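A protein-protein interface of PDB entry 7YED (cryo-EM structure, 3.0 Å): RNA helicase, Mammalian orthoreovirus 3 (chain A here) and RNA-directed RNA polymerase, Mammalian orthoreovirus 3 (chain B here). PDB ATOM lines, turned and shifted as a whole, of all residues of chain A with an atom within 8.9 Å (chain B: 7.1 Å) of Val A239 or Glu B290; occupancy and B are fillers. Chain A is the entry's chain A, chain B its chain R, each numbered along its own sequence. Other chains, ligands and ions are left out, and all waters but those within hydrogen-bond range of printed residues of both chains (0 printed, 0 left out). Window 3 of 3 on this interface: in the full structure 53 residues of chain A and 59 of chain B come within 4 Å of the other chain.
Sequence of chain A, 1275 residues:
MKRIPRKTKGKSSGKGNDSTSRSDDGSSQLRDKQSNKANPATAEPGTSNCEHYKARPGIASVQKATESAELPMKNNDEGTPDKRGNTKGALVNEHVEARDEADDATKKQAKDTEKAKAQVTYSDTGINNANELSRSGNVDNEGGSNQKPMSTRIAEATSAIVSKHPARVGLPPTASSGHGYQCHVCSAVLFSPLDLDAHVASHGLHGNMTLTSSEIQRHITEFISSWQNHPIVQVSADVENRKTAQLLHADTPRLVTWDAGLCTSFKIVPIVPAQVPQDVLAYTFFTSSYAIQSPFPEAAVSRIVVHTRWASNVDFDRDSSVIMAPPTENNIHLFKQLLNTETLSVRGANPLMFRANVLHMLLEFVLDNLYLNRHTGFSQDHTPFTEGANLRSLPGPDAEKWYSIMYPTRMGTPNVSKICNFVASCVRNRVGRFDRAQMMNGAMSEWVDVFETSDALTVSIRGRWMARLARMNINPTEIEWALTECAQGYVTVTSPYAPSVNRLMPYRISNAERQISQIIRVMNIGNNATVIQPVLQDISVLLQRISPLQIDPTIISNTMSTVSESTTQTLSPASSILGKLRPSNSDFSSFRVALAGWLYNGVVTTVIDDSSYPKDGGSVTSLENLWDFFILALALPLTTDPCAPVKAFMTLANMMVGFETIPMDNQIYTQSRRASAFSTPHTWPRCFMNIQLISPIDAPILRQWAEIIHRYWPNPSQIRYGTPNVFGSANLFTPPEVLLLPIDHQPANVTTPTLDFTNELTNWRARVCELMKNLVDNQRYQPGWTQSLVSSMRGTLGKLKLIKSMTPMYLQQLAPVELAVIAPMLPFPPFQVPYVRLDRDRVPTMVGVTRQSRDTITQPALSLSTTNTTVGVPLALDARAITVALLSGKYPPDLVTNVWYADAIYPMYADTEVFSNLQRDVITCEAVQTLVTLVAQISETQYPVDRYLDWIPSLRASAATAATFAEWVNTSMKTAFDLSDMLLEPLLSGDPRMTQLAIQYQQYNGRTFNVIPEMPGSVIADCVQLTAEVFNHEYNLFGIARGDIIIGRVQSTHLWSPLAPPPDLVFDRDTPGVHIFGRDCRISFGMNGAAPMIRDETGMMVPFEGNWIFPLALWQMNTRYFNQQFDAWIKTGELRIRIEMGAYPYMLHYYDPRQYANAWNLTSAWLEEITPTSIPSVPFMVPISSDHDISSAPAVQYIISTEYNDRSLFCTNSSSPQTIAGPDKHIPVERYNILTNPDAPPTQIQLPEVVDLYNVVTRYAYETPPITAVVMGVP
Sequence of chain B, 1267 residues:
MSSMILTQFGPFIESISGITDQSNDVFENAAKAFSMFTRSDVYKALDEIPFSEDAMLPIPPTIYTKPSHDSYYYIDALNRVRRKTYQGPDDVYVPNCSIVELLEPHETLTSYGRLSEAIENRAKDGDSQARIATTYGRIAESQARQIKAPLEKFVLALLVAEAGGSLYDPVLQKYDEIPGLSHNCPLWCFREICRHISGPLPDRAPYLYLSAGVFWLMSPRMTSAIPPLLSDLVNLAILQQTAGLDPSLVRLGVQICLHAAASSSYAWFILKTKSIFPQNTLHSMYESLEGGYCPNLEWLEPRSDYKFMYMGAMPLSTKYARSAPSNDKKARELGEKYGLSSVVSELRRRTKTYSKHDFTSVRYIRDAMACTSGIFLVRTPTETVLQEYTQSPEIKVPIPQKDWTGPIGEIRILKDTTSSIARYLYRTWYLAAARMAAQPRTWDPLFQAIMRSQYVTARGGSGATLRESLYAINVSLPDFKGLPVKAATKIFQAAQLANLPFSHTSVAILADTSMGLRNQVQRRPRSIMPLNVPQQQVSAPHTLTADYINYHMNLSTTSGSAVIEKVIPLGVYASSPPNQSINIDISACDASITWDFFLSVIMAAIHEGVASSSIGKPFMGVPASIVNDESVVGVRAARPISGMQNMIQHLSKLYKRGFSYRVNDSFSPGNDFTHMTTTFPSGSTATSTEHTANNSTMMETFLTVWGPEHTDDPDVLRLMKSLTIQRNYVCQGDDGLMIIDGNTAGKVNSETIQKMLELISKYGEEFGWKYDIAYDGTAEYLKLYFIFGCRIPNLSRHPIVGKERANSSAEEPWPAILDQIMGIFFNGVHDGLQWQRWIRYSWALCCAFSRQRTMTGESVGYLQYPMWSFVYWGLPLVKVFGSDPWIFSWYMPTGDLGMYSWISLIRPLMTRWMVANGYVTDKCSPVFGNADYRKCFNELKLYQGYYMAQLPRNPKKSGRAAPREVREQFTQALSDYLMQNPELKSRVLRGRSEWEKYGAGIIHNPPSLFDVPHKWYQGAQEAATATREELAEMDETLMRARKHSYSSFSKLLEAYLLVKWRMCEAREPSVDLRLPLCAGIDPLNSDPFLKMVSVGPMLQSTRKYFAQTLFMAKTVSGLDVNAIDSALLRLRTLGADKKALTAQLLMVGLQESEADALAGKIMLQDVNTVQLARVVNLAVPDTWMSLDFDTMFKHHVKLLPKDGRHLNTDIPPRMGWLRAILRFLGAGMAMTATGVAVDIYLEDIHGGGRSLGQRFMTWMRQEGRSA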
ATOM      1  N   SER A 236     -13.076  28.992   9.775  1.00  0.00           N
ATOM      2  CA  SER A 236     -14.176  28.213   9.223  1.00  0.00           C
ATOM      3  C   SER A 236     -14.550  27.129  10.222  1.00  0.00           C
ATOM      4  O   SER A 236     -13.731  26.711  11.044  1.00  0.00           O
ATOM      5  CB  SER A 236     -13.815  27.586   7.878  1.00  0.00           C
ATOM      6  OG  SER A 236     -12.800  26.615   8.036  1.00  0.00           O
ATOM      7  N   ALA A 237     -15.798  26.677  10.136  1.00  0.00           N
ATOM      8  CA  ALA A 237     -16.283  25.607  10.992  1.00  0.00           C
ATOM      9  C   ALA A 237     -17.564  25.053  10.394  1.00  0.00           C
ATOM     10  O   ALA A 237     -18.206  25.691   9.556  1.00  0.00           O
ATOM     11  CB  ALA A 237     -16.523  26.090  12.425  1.00  0.00           C
ATOM     12  N   ASP A 238     -17.931  23.853  10.838  1.00  0.00           N
ATOM     13  CA  ASP A 238     -19.135  23.184  10.362  1.00  0.00           C
ATOM     14  C   ASP A 238     -20.288  23.250  11.352  1.00  0.00           C
ATOM     15  O   ASP A 238     -21.440  23.415  10.943  1.00  0.00           O
ATOM     16  CB  ASP A 238     -18.830  21.720  10.028  1.00  0.00           C
ATOM     17  CG  ASP A 238     -18.329  20.935  11.227  1.00  0.00           C
ATOM     18  OD1 ASP A 238     -18.142  21.532  12.307  1.00  0.00           O
ATOM     19  OD2 ASP A 238     -18.122  19.713  11.089  1.00  0.00           O
ATOM     20  N   VAL A 239     -20.006  23.127  12.639  1.00  0.00           N
ATOM     21  CA  VAL A 239     -21.036  23.063  13.667  1.00  0.00           C
ATOM     22  C   VAL A 239     -21.277  24.458  14.218  1.00  0.00           C
ATOM     23  O   VAL A 239     -20.341  25.244  14.400  1.00  0.00           O
ATOM     24  CB  VAL A 239     -20.628  22.085  14.785  1.00  0.00           C
ATOM     25  CG1 VAL A 239     -19.396  22.598  15.508  1.00  0.00           C
ATOM     26  CG2 VAL A 239     -21.777  21.878  15.754  1.00  0.00           C
ATOM     27  N   GLU A 240     -22.541  24.768  14.488  1.00  0.00           N
ATOM     28  CA  GLU A 240     -22.914  26.091  14.960  1.00  0.00           C
ATOM     29  C   GLU A 240     -22.667  26.227  16.457  1.00  0.00           C
ATOM     30  O   GLU A 240     -22.754  25.259  17.216  1.00  0.00           O
ATOM     31  CB  GLU A 240     -24.385  26.372  14.660  1.00  0.00           C
ATOM     32  CG  GLU A 240     -24.712  26.456  13.184  1.00  0.00           C
ATOM     33  CD  GLU A 240     -24.045  27.637  12.517  1.00  0.00           C
ATOM     34  OE1 GLU A 240     -23.840  28.659  13.198  1.00  0.00           O
ATOM     35  OE2 GLU A 240     -23.729  27.549  11.313  1.00  0.00           O
ATOM     36  N   ASN A 241     -22.356  27.447  16.876  1.00  0.00           N
ATOM     37  CA  ASN A 241     -22.224  27.766  18.286  1.00  0.00           C
ATOM     38  C   ASN A 241     -23.536  28.329  18.819  1.00  0.00           C
ATOM     39  O   ASN A 241     -24.454  28.654  18.065  1.00  0.00           O
ATOM     40  CB  ASN A 241     -21.093  28.767  18.512  1.00  0.00           C
ATOM     41  CG  ASN A 241     -19.748  28.219  18.112  1.00  0.00           C
ATOM     42  OD1 ASN A 241     -19.122  28.709  17.175  1.00  0.00           O
ATOM     43  ND2 ASN A 241     -19.291  27.192  18.818  1.00  0.00           N
ATOM     44  N   ARG A 242     -23.612  28.444  20.145  1.00  0.00           N
ATOM     45  CA  ARG A 242     -24.796  29.029  20.760  1.00  0.00           C
ATOM     46  C   ARG A 242     -25.007  30.460  20.287  1.00  0.00           C
ATOM     47  O   ARG A 242     -26.131  30.855  19.962  1.00  0.00           O
ATOM     48  CB  ARG A 242     -24.677  28.985  22.281  1.00  0.00           C
ATOM     49  CG  ARG A 242     -24.727  27.591  22.870  1.00  0.00           C
ATOM     50  CD  ARG A 242     -24.600  27.635  24.384  1.00  0.00           C
ATOM     51  NE  ARG A 242     -24.676  26.304  24.976  1.00  0.00           N
ATOM     52  CZ  ARG A 242     -23.622  25.527  25.207  1.00  0.00           C
ATOM     53  NH1 ARG A 242     -22.403  25.947  24.896  1.00  0.00           N
ATOM     54  NH2 ARG A 242     -23.787  24.329  25.748  1.00  0.00           N
ATOM     55  N   THR A 244     -23.853  32.013  17.501  1.00  0.00           N
ATOM     56  CA  THR A 244     -24.201  32.116  16.089  1.00  0.00           C
ATOM     57  C   THR A 244     -25.616  31.623  15.835  1.00  0.00           C
ATOM     58  O   THR A 244     -26.330  32.183  14.997  1.00  0.00           O
ATOM     59  CB  THR A 244     -23.209  31.339  15.235  1.00  0.00           C
ATOM     60  OG1 THR A 244     -21.883  31.811  15.497  1.00  0.00           O
ATOM     61  CG2 THR A 244     -23.518  31.553  13.770  1.00  0.00           C
ATOM     62  N   ALA A 245     -26.042  30.573  16.540  1.00  0.00           N
ATOM     63  CA  ALA A 245     -27.419  30.118  16.399  1.00  0.00           C
ATOM     64  C   ALA A 245     -28.397  31.166  16.909  1.00  0.00           C
ATOM     65  O   ALA A 245     -29.437  31.406  16.287  1.00  0.00           O
ATOM     66  CB  ALA A 245     -27.614  28.794  17.135  1.00  0.00           C
ATOM     67  N   THR A 530     -15.761  34.058  14.893  1.00  0.00           N
ATOM     68  CA  THR A 530     -16.421  32.795  14.604  1.00  0.00           C
ATOM     69  C   THR A 530     -17.923  32.900  14.770  1.00  0.00           C
ATOM     70  O   THR A 530     -18.629  31.905  14.596  1.00  0.00           O
ATOM     71  CB  THR A 530     -15.886  31.680  15.502  1.00  0.00           C
ATOM     72  OG1 THR A 530     -16.193  31.980  16.867  1.00  0.00           O
ATOM     73  CG2 THR A 530     -14.386  31.550  15.346  1.00  0.00           C
ATOM     74  N   GLN A 533     -18.521  35.032  10.853  1.00  0.00           N
ATOM     75  CA  GLN A 533     -18.179  34.363   9.599  1.00  0.00           C
ATOM     76  C   GLN A 533     -19.354  33.603   8.998  1.00  0.00           C
ATOM     77  O   GLN A 533     -19.585  33.733   7.781  1.00  0.00           O
ATOM     78  CB  GLN A 533     -16.977  33.443   9.825  1.00  0.00           C
ATOM     79  CG  GLN A 533     -16.374  32.854   8.558  1.00  0.00           C
ATOM     80  CD  GLN A 533     -17.026  31.549   8.149  1.00  0.00           C
ATOM     81  OE1 GLN A 533     -17.526  30.803   8.988  1.00  0.00           O
ATOM     82  NE2 GLN A 533     -17.025  31.269   6.854  1.00  0.00           N
ATOM     83  N   PRO A 534     -20.106  32.791   9.747  1.00  0.00           N
ATOM     84  CA  PRO A 534     -21.212  32.046   9.126  1.00  0.00           C
ATOM     85  C   PRO A 534     -22.281  32.924   8.503  1.00  0.00           C
ATOM     86  O   PRO A 534     -22.889  32.520   7.504  1.00  0.00           O
ATOM     87  CB  PRO A 534     -21.768  31.223  10.294  1.00  0.00           C
ATOM     88  CG  PRO A 534     -20.615  31.065  11.210  1.00  0.00           C
ATOM     89  CD  PRO A 534     -19.856  32.341  11.127  1.00  0.00           C
ATOM     90  N   TYR B 286     -28.753  10.475   7.566  1.00  0.00           N
ATOM     91  CA  TYR B 286     -28.825  11.889   7.917  1.00  0.00           C
ATOM     92  C   TYR B 286     -30.266  12.381   8.044  1.00  0.00           C
ATOM     93  O   TYR B 286     -30.702  13.305   7.359  1.00  0.00           O
ATOM     94  CB  TYR B 286     -28.042  12.729   6.907  1.00  0.00           C
ATOM     95  CG  TYR B 286     -26.574  12.411   6.937  1.00  0.00           C
ATOM     96  CD1 TYR B 286     -25.779  12.866   7.967  1.00  0.00           C
ATOM     97  CD2 TYR B 286     -25.986  11.652   5.941  1.00  0.00           C
ATOM     98  CE1 TYR B 286     -24.443  12.576   8.011  1.00  0.00           C
ATOM     99  CE2 TYR B 286     -24.645  11.355   5.976  1.00  0.00           C
ATOM    100  CZ  TYR B 286     -23.881  11.822   7.014  1.00  0.00           C
ATOM    101  OH  TYR B 286     -22.541  11.536   7.065  1.00  0.00           O
ATOM    102  N   SER B 288     -30.746  13.784  10.732  1.00  0.00           N
ATOM    103  CA  SER B 288     -30.410  14.902  11.609  1.00  0.00           C
ATOM    104  C   SER B 288     -28.967  15.293  11.328  1.00  0.00           C
ATOM    105  O   SER B 288     -28.049  14.555  11.692  1.00  0.00           O
ATOM    106  CB  SER B 288     -30.603  14.515  13.068  1.00  0.00           C
ATOM    107  OG  SER B 288     -31.961  14.215  13.334  1.00  0.00           O
ATOM    108  N   LEU B 289     -28.768  16.439  10.686  1.00  0.00           N
ATOM    109  CA  LEU B 289     -27.428  16.928  10.413  1.00  0.00           C
ATOM    110  C   LEU B 289     -26.913  17.784  11.559  1.00  0.00           C
ATOM    111  O   LEU B 289     -27.677  18.376  12.324  1.00  0.00           O
ATOM    112  CB  LEU B 289     -27.379  17.752   9.129  1.00  0.00           C
ATOM    113  CG  LEU B 289     -27.502  17.058   7.784  1.00  0.00           C
ATOM    114  CD1 LEU B 289     -27.568  18.096   6.693  1.00  0.00           C
ATOM    115  CD2 LEU B 289     -26.315  16.163   7.568  1.00  0.00           C
ATOM    116  N   GLU B 290     -25.590  17.841  11.664  1.00  0.00           N
ATOM    117  CA  GLU B 290     -24.932  18.754  12.584  1.00  0.00           C
ATOM    118  C   GLU B 290     -23.735  19.462  11.978  1.00  0.00           C
ATOM    119  O   GLU B 290     -23.256  20.428  12.578  1.00  0.00           O
ATOM    120  CB  GLU B 290     -24.484  18.010  13.846  1.00  0.00           C
ATOM    121  CG  GLU B 290     -25.632  17.478  14.679  1.00  0.00           C
ATOM    122  CD  GLU B 290     -26.485  18.584  15.263  1.00  0.00           C
ATOM    123  OE1 GLU B 290     -25.939  19.672  15.549  1.00  0.00           O
ATOM    124  OE2 GLU B 290     -27.702  18.369  15.439  1.00  0.00           O
ATOM    125  N   GLY B 291     -23.236  19.034  10.830  1.00  0.00           N
ATOM    126  CA  GLY B 291     -22.060  19.643  10.251  1.00  0.00           C
ATOM    127  C   GLY B 291     -21.471  18.748   9.180  1.00  0.00           C
ATOM    128  O   GLY B 291     -22.041  17.720   8.819  1.00  0.00           O
ATOM    129  N   GLY B 292     -20.315  19.162   8.691  1.00  0.00           N
ATOM    130  CA  GLY B 292     -19.659  18.492   7.592  1.00  0.00           C
ATOM    131  C   GLY B 292     -19.658  19.346   6.336  1.00  0.00           C
ATOM    132  O   GLY B 292     -20.414  20.309   6.197  1.00  0.00           O
ATOM    133  N   TYR B 293     -18.791  18.974   5.404  1.00  0.00           N
ATOM    134  CA  TYR B 293     -18.570  19.749   4.195  1.00  0.00           C
ATOM    135  C   TYR B 293     -19.018  18.966   2.972  1.00  0.00           C
ATOM    136  O   TYR B 293     -18.829  17.750   2.900  1.00  0.00           O
ATOM    137  CB  TYR B 293     -17.096  20.121   4.056  1.00  0.00           C
ATOM    138  CG  TYR B 293     -16.616  21.095   5.099  1.00  0.00           C
ATOM    139  CD1 TYR B 293     -17.512  21.831   5.851  1.00  0.00           C
ATOM    140  CD2 TYR B 293     -15.269  21.271   5.339  1.00  0.00           C
ATOM    141  CE1 TYR B 293     -17.078  22.718   6.808  1.00  0.00           C
ATOM    142  CE2 TYR B 293     -14.827  22.156   6.288  1.00  0.00           C
ATOM    143  CZ  TYR B 293     -15.734  22.875   7.022  1.00  0.00           C
ATOM    144  OH  TYR B 293     -15.292  23.758   7.973  1.00  0.00           O
ATOM    145  N   PRO B 315     -19.860  24.541   4.147  1.00  0.00           N
ATOM    146  CA  PRO B 315     -20.256  23.792   5.343  1.00  0.00           C
ATOM    147  C   PRO B 315     -21.745  23.492   5.347  1.00  0.00           C
ATOM    148  O   PRO B 315     -22.564  24.313   4.931  1.00  0.00           O
ATOM    149  CB  PRO B 315     -19.873  24.731   6.489  1.00  0.00           C
ATOM    150  CG  PRO B 315     -19.916  26.082   5.885  1.00  0.00           C
ATOM    151  CD  PRO B 315     -19.471  25.923   4.463  1.00  0.00           C
ATOM    152  N   LEU B 316     -22.089  22.300   5.823  1.00  0.00           N
ATOM    153  CA  LEU B 316     -23.480  21.894   5.925  1.00  0.00           C
ATOM    154  C   LEU B 316     -24.099  22.442   7.206  1.00  0.00           C
ATOM    155  O   LEU B 316     -23.406  22.909   8.113  1.00  0.00           O
ATOM    156  CB  LEU B 316     -23.598  20.373   5.886  1.00  0.00           C
ATOM    157  CG  LEU B 316     -23.205  19.701   4.573  1.00  0.00           C
ATOM    158  CD1 LEU B 316     -23.230  18.199   4.724  1.00  0.00           C
ATOM    159  CD2 LEU B 316     -24.134  20.136   3.463  1.00  0.00           C
ATOM    160  N   SER B 317     -25.423  22.377   7.280  1.00  0.00           N
ATOM    161  CA  SER B 317     -26.144  22.888   8.437  1.00  0.00           C
ATOM    162  C   SER B 317     -27.402  22.055   8.646  1.00  0.00           C
ATOM    163  O   SER B 317     -27.645  21.068   7.949  1.00  0.00           O
ATOM    164  CB  SER B 317     -26.484  24.368   8.265  1.00  0.00           C
ATOM    165  OG  SER B 317     -27.411  24.555   7.212  1.00  0.00           O
ATOM    166  N   THR B 318     -28.210  22.472   9.621  1.00  0.00           N
ATOM    167  CA  THR B 318     -29.401  21.709   9.972  1.00  0.00           C
ATOM    168  C   THR B 318     -30.463  21.780   8.887  1.00  0.00           C
ATOM    169  O   THR B 318     -31.274  20.859   8.753  1.00  0.00           O
ATOM    170  CB  THR B 318     -29.968  22.215  11.296  1.00  0.00           C
ATOM    171  OG1 THR B 318     -28.980  22.079  12.323  1.00  0.00           O
ATOM    172  CG2 THR B 318     -31.198  21.418  11.684  1.00  0.00           C
ATOM    173  N   SER B 355     -24.614  11.723  12.458  1.00  0.00           N
ATOM    174  CA  SER B 355     -25.239  13.025  12.264  1.00  0.00           C
ATOM    175  C   SER B 355     -24.235  14.054  11.765  1.00  0.00           C
ATOM    176  O   SER B 355     -24.382  15.249  12.027  1.00  0.00           O
ATOM    177  CB  SER B 355     -25.895  13.509  13.554  1.00  0.00           C
ATOM    178  OG  SER B 355     -24.919  13.763  14.546  1.00  0.00           O
ATOM    179  N   LYS B 356     -23.211  13.610  11.044  1.00  0.00           N
ATOM    180  CA  LYS B 356     -22.205  14.519  10.510  1.00  0.00           C
ATOM    181  C   LYS B 356     -21.651  13.923   9.229  1.00  0.00           C
ATOM    182  O   LYS B 356     -21.152  12.796   9.241  1.00  0.00           O
ATOM    183  CB  LYS B 356     -21.081  14.750  11.517  1.00  0.00           C
ATOM    184  CG  LYS B 356     -21.480  15.580  12.717  1.00  0.00           C
ATOM    185  CD  LYS B 356     -20.345  15.673  13.715  1.00  0.00           C
ATOM    186  CE  LYS B 356     -19.464  16.870  13.422  1.00  0.00           C
ATOM    187  NZ  LYS B 356     -18.685  16.676  12.169  1.00  0.00           N
ATOM    188  N   HIS B 357     -21.735  14.667   8.132  1.00  0.00           N
ATOM    189  CA  HIS B 357     -21.154  14.203   6.880  1.00  0.00           C
ATOM    190  C   HIS B 357     -19.642  14.166   7.035  1.00  0.00           C
ATOM    191  O   HIS B 357     -18.979  15.205   7.020  1.00  0.00           O
ATOM    192  CB  HIS B 357     -21.570  15.104   5.725  1.00  0.00           C
ATOM    193  CG  HIS B 357     -21.079  14.633   4.395  1.00  0.00           C
ATOM    194  ND1 HIS B 357     -21.608  13.535   3.753  1.00  0.00           N
ATOM    195  CD2 HIS B 357     -20.105  15.109   3.585  1.00  0.00           C
ATOM    196  CE1 HIS B 357     -20.982  13.355   2.605  1.00  0.00           C
ATOM    197  NE2 HIS B 357     -20.066  14.298   2.478  1.00  0.00           N
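Hydrophobic or aromatic side chains of chain A that line the printed part of chain B: Val A239. Of the 14 printed residues of chain B, 7 touch a printed residue of chain A. Hydrophobic or aromatic side chains of chain B that line the printed part of chain A: Tyr B293 and Pro B315. Among the printed residues, Asp or Glu carboxylates within 4 Å of a Lys or Arg side-chain nitrogen of the other chain: Asp A238 with Lys B356 (3.3 Å).
Tyr B293 touches Ser A236 (OH to OG, 3.8 Å). Ala A237 touches Tyr B293 (C to OH, 3.6 Å). Ala A237 touches Pro B315 (O to CB, 3.6 Å). O of Glu B290 touches O of Asp A238 (3.9 Å). Gly B291 touches Asp A238 (CA to CB, 3.8 Å). CB of Asp A238 touches CE1 of Tyr B293 (3.8 Å). CA of Val A239 touches O of Glu B290 (3.6 Å).
Of the printed residues of chain B, Ala A237 touches Tyr B293 (3.6 Å) and Pro B315 (3.6 Å). Of chain B, only Glu B290 comes within 4 Å of Val A239. Pro A534 touches none of the printed residues of chain B. Printed residues of chain A within 4 Å of Glu B290: Asp A238 and Val A239. Gly B291 touches just one residue of chain A: Asp A238. Printed residues of chain A within 4 Å of Gly B292: Asp A238 (3.2 Å). Of the printed residues of chain A, Pro B315 touches Ala A237. Ser B317 touches none of the printed residues of chain A. Of the printed residues of chain A, Lys B356 touches Asp A238 (3.3 Å). The nearest printed residue of chain B that does not touch Ser A236 is Pro B315 (6.6 Å).
The side-chain carboxylate (OD2) of Asp A238 lies close to the backbone NH (N) of Gly B292, at 3.3 Å. The side-chain carboxylate of Asp A238 is in salt-bridge range of the side-chain amino group of Lys B356. O of Asp A238 lies close to O of Leu B316 (3.5 Å).
The backbone carbonyl oxygen (O) of Ser B355 sits at hydrogen-bond distance from the backbone NH (N) of Glu B290 (2.9 Å). O of Lys B356 sits at hydrogen-bond distance from OH of Tyr B286 (2.9 Å). O of Gly B292 sits at hydrogen-bond distance from N of Leu B316 (2.6 Å). The backbone carbonyl oxygen (O) of Gly B291 is in hydrogen-bond range of the backbone NH (N) of His B357 (3.1 Å).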
